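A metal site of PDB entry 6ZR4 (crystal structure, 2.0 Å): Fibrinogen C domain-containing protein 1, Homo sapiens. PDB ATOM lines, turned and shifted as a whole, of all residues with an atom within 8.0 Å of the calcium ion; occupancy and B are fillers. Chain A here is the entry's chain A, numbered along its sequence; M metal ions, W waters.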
ATOM      1  N   THR A 153       9.982   9.441 -28.614  1.00  0.00           N
ATOM      2  CA  THR A 153       8.894   8.661 -27.980  1.00  0.00           C
ATOM      3  C   THR A 153       8.141   9.557 -26.987  1.00  0.00           C
ATOM      4  O   THR A 153       8.802  10.236 -26.175  1.00  0.00           O
ATOM      5  CB  THR A 153       9.435   7.380 -27.338  1.00  0.00           C
ATOM      6  OG1 THR A 153       9.637   6.428 -28.376  1.00  0.00           O
ATOM      7  CG2 THR A 153       8.509   6.808 -26.291  1.00  0.00           C
ATOM      8  N   ARG A 157       2.883   7.447 -28.027  1.00  0.00           N
ATOM      9  CA  ARG A 157       3.557   6.987 -29.274  1.00  0.00           C
ATOM     10  C   ARG A 157       4.942   6.431 -28.943  1.00  0.00           C
ATOM     11  O   ARG A 157       5.917   7.213 -28.877  1.00  0.00           O
ATOM     12  CB  ARG A 157       3.623   8.108 -30.323  1.00  0.00           C
ATOM     13  CG  ARG A 157       3.872   7.594 -31.730  1.00  0.00           C
ATOM     14  CD  ARG A 157       3.899   8.735 -32.736  1.00  0.00           C
ATOM     15  NE  ARG A 157       3.952   8.274 -34.123  1.00  0.00           N
ATOM     16  CZ  ARG A 157       5.048   7.910 -34.763  1.00  0.00           C
ATOM     17  NH1 ARG A 157       6.230   7.911 -34.151  1.00  0.00           N
ATOM     18  NH2 ARG A 157       4.973   7.523 -36.033  1.00  0.00           N
ATOM     19  N   ASP A 158       4.994   5.108 -28.806  1.00  0.00           N
ATOM     20  CA  ASP A 158       6.165   4.321 -28.341  1.00  0.00           C
ATOM     21  C   ASP A 158       6.996   3.871 -29.548  1.00  0.00           C
ATOM     22  O   ASP A 158       6.513   3.019 -30.295  1.00  0.00           O
ATOM     23  CB  ASP A 158       5.663   3.127 -27.515  1.00  0.00           C
ATOM     24  CG  ASP A 158       6.768   2.287 -26.911  1.00  0.00           C
ATOM     25  OD1 ASP A 158       7.911   2.407 -27.382  1.00  0.00           O
ATOM     26  OD2 ASP A 158       6.472   1.531 -25.974  1.00  0.00           O
ATOM     27  N   SER A 159       8.209   4.408 -29.702  1.00  0.00           N
ATOM     28  CA  SER A 159       9.186   3.995 -30.736  1.00  0.00           C
ATOM     29  C   SER A 159      10.531   3.635 -30.089  1.00  0.00           C
ATOM     30  O   SER A 159      11.539   3.654 -30.811  1.00  0.00           O
ATOM     31  CB  SER A 159       9.371   5.056 -31.784  1.00  0.00           C
ATOM     32  OG  SER A 159       8.123   5.405 -32.368  1.00  0.00           O
ATOM     33  N   ASP A 160      10.552   3.324 -28.785  1.00  0.00           N
ATOM     34  CA  ASP A 160      11.807   3.110 -28.024  1.00  0.00           C
ATOM     35  C   ASP A 160      12.223   1.630 -28.123  1.00  0.00           C
ATOM     36  O   ASP A 160      11.482   0.860 -28.780  1.00  0.00           O
ATOM     37  CB  ASP A 160      11.657   3.593 -26.578  1.00  0.00           C
ATOM     38  CG  ASP A 160      10.574   2.882 -25.777  1.00  0.00           C
ATOM     39  OD1 ASP A 160      10.501   1.627 -25.872  1.00  0.00           O
ATOM     40  OD2 ASP A 160       9.805   3.573 -25.074  1.00  0.00           O
ATOM     41  N   HIS A 161      13.363   1.250 -27.529  1.00  0.00           N
ATOM     42  CA  HIS A 161      13.874  -0.146 -27.476  1.00  0.00           C
ATOM     43  C   HIS A 161      13.581  -0.771 -26.112  1.00  0.00           C
ATOM     44  O   HIS A 161      14.357  -1.636 -25.678  1.00  0.00           O
ATOM     45  CB  HIS A 161      15.377  -0.203 -27.789  1.00  0.00           C
ATOM     46  CG  HIS A 161      15.726   0.163 -29.192  1.00  0.00           C
ATOM     47  ND1 HIS A 161      14.759   0.476 -30.137  1.00  0.00           N
ATOM     48  CD2 HIS A 161      16.920   0.268 -29.814  1.00  0.00           C
ATOM     49  CE1 HIS A 161      15.350   0.763 -31.284  1.00  0.00           C
ATOM     50  NE2 HIS A 161      16.670   0.647 -31.117  1.00  0.00           N
ATOM     51  N   SER A 162      12.502  -0.343 -25.445  1.00  0.00           N
ATOM     52  CA  SER A 162      12.035  -0.925 -24.155  1.00  0.00           C
ATOM     53  C   SER A 162      10.758  -1.728 -24.416  1.00  0.00           C
ATOM     54  O   SER A 162      10.027  -1.364 -25.357  1.00  0.00           O
ATOM     55  CB  SER A 162      11.810   0.146 -23.127  1.00  0.00           C
ATOM     56  OG  SER A 162      11.206  -0.409 -21.970  1.00  0.00           O
ATOM     57  N   GLU A 163      10.506  -2.764 -23.607  1.00  0.00           N
ATOM     58  CA  GLU A 163       9.246  -3.556 -23.640  1.00  0.00           C
ATOM     59  C   GLU A 163       8.119  -2.697 -23.062  1.00  0.00           C
ATOM     60  O   GLU A 163       6.946  -2.988 -23.367  1.00  0.00           O
ATOM     61  CB  GLU A 163       9.411  -4.856 -22.854  1.00  0.00           C
ATOM     62  CG  GLU A 163      10.446  -5.800 -23.453  1.00  0.00           C
ATOM     63  CD  GLU A 163      10.146  -6.306 -24.853  1.00  0.00           C
ATOM     64  OE1 GLU A 163       8.964  -6.254 -25.260  1.00  0.00           O
ATOM     65  OE2 GLU A 163      11.092  -6.750 -25.540  1.00  0.00           O
ATOM     66  N   ASN A 164       8.469  -1.673 -22.280  1.00  0.00           N
ATOM     67  CA  ASN A 164       7.531  -0.635 -21.771  1.00  0.00           C
ATOM     68  C   ASN A 164       7.631   0.625 -22.643  1.00  0.00           C
ATOM     69  O   ASN A 164       8.421   0.629 -23.618  1.00  0.00           O
ATOM     70  CB  ASN A 164       7.815  -0.309 -20.303  1.00  0.00           C
ATOM     71  CG  ASN A 164       7.914  -1.558 -19.463  1.00  0.00           C
ATOM     72  OD1 ASN A 164       6.893  -2.189 -19.178  1.00  0.00           O
ATOM     73  ND2 ASN A 164       9.124  -1.950 -19.097  1.00  0.00           N
ATOM     74  N   ASN A 165       6.832   1.634 -22.299  1.00  0.00           N
ATOM     75  CA  ASN A 165       6.888   2.999 -22.886  1.00  0.00           C
ATOM     76  C   ASN A 165       7.754   3.852 -21.953  1.00  0.00           C
ATOM     77  O   ASN A 165       7.263   4.215 -20.874  1.00  0.00           O
ATOM     78  CB  ASN A 165       5.486   3.573 -23.104  1.00  0.00           C
ATOM     79  CG  ASN A 165       5.507   4.922 -23.800  1.00  0.00           C
ATOM     80  OD1 ASN A 165       6.376   5.749 -23.525  1.00  0.00           O
ATOM     81  ND2 ASN A 165       4.551   5.148 -24.684  1.00  0.00           N
ATOM     82  N   CYS A 166       8.983   4.134 -22.365  1.00  0.00           N
ATOM     83  CA  CYS A 166       9.984   4.911 -21.586  1.00  0.00           C
ATOM     84  C   CYS A 166       9.408   6.269 -21.173  1.00  0.00           C
ATOM     85  O   CYS A 166       9.698   6.693 -20.032  1.00  0.00           O
ATOM     86  CB  CYS A 166      11.271   5.125 -22.389  1.00  0.00           C
ATOM     87  SG  CYS A 166      12.245   3.617 -22.621  1.00  0.00           S
ATOM     88  N   ALA A 167       8.659   6.923 -22.069  1.00  0.00           N
ATOM     89  CA  ALA A 167       8.075   8.269 -21.855  1.00  0.00           C
ATOM     90  C   ALA A 167       7.058   8.220 -20.693  1.00  0.00           C
ATOM     91  O   ALA A 167       7.068   9.141 -19.861  1.00  0.00           O
ATOM     92  CB  ALA A 167       7.414   8.766 -23.119  1.00  0.00           C
ATOM     93  N   TYR A 176      14.238   8.155 -26.539  1.00  0.00           N
ATOM     94  CA  TYR A 176      14.479   7.082 -25.550  1.00  0.00           C
ATOM     95  C   TYR A 176      15.048   5.850 -26.265  1.00  0.00           C
ATOM     96  O   TYR A 176      14.597   5.521 -27.389  1.00  0.00           O
ATOM     97  CB  TYR A 176      13.188   6.738 -24.810  1.00  0.00           C
ATOM     98  CG  TYR A 176      12.693   7.786 -23.854  1.00  0.00           C
ATOM     99  CD1 TYR A 176      13.413   8.103 -22.709  1.00  0.00           C
ATOM    100  CD2 TYR A 176      11.471   8.409 -24.035  1.00  0.00           C
ATOM    101  CE1 TYR A 176      12.944   9.052 -21.798  1.00  0.00           C
ATOM    102  CE2 TYR A 176      10.970   9.334 -23.135  1.00  0.00           C
ATOM    103  CZ  TYR A 176      11.718   9.655 -22.014  1.00  0.00           C
ATOM    104  OH  TYR A 176      11.238  10.582 -21.126  1.00  0.00           O
ATOM    105  N   ARG A 177      16.016   5.199 -25.627  1.00  0.00           N
ATOM    106  CA  ARG A 177      16.512   3.850 -26.021  1.00  0.00           C
ATOM    107  C   ARG A 177      15.904   2.844 -25.039  1.00  0.00           C
ATOM    108  O   ARG A 177      14.770   2.394 -25.285  1.00  0.00           O
ATOM    109  CB  ARG A 177      18.043   3.855 -26.081  1.00  0.00           C
ATOM    110  CG  ARG A 177      18.643   2.554 -26.577  1.00  0.00           C
ATOM    111  CD  ARG A 177      20.151   2.605 -26.665  1.00  0.00           C
ATOM    112  NE  ARG A 177      20.606   3.620 -27.611  1.00  0.00           N
ATOM    113  CZ  ARG A 177      20.788   3.432 -28.918  1.00  0.00           C
ATOM    114  NH1 ARG A 177      20.561   2.267 -29.488  1.00  0.00           N
ATOM    115  NH2 ARG A 177      21.209   4.452 -29.664  1.00  0.00           N
ATOM    116  N   ASN A 178      16.596   2.550 -23.940  1.00  0.00           N
ATOM    117  CA  ASN A 178      16.144   1.565 -22.927  1.00  0.00           C
ATOM    118  C   ASN A 178      16.796   1.875 -21.576  1.00  0.00           C
ATOM    119  O   ASN A 178      17.494   1.009 -21.047  1.00  0.00           O
ATOM    120  CB  ASN A 178      16.457   0.144 -23.417  1.00  0.00           C
ATOM    121  CG  ASN A 178      15.795  -0.926 -22.573  1.00  0.00           C
ATOM    122  OD1 ASN A 178      14.707  -0.730 -22.054  1.00  0.00           O
ATOM    123  ND2 ASN A 178      16.453  -2.069 -22.447  1.00  0.00           N
ATOM    124  N   CYS A 179      16.572   3.060 -21.009  1.00  0.00           N
ATOM    125  CA  CYS A 179      15.658   4.080 -21.526  1.00  0.00           C
ATOM    126  C   CYS A 179      16.398   5.390 -21.800  1.00  0.00           C
ATOM    127  O   CYS A 179      16.216   5.915 -22.914  1.00  0.00           O
ATOM    128  CB  CYS A 179      14.499   4.340 -20.574  1.00  0.00           C
ATOM    129  SG  CYS A 179      13.118   3.185 -20.781  1.00  0.00           S
HETATM  130 CA    CA M   1       8.597   0.427 -25.985  1.00  0.00          CA
HETATM  131  O   HOH W   1       7.034  -1.362 -26.163  1.00  0.00           O
HETATM  132  O   HOH W   2       9.259  -0.236 -28.137  1.00  0.00           O
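The backbone NH (N) of Asn 164 is in hydrogen-bond range of the side-chain hydroxyl (OG) of Ser 162.
The side-chain carboxylate (OD2) of Asp 160 lies within hydrogen-bond range of the backbone NH (N) of Cys 166 (2.9 Å).
SG of Cys 179 forms a disulfide with SG of Cys 166, 2.1 Å away.
The side-chain hydroxyl (OG1) of Thr 153 lies within hydrogen-bond range of the backbone NH (N) of Asp 160 (3.3 Å).
The calcium ion is bound by OD1 of Asp 160 (2.3 Å), water W2 (2.3 Å), O of Ser 162 (2.4 Å), water W1 (2.4 Å), O of Asn 164 (2.4 Å), OD2 of Asp 158 (2.4 Å) and OD1 of Asp 158 (2.5 Å).
Of the 16 residues printed, 4 come within 4 Å of the calcium ion.
The nearest printed residue that does not touch the calcium ion is Asn 165 (4.3 Å).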
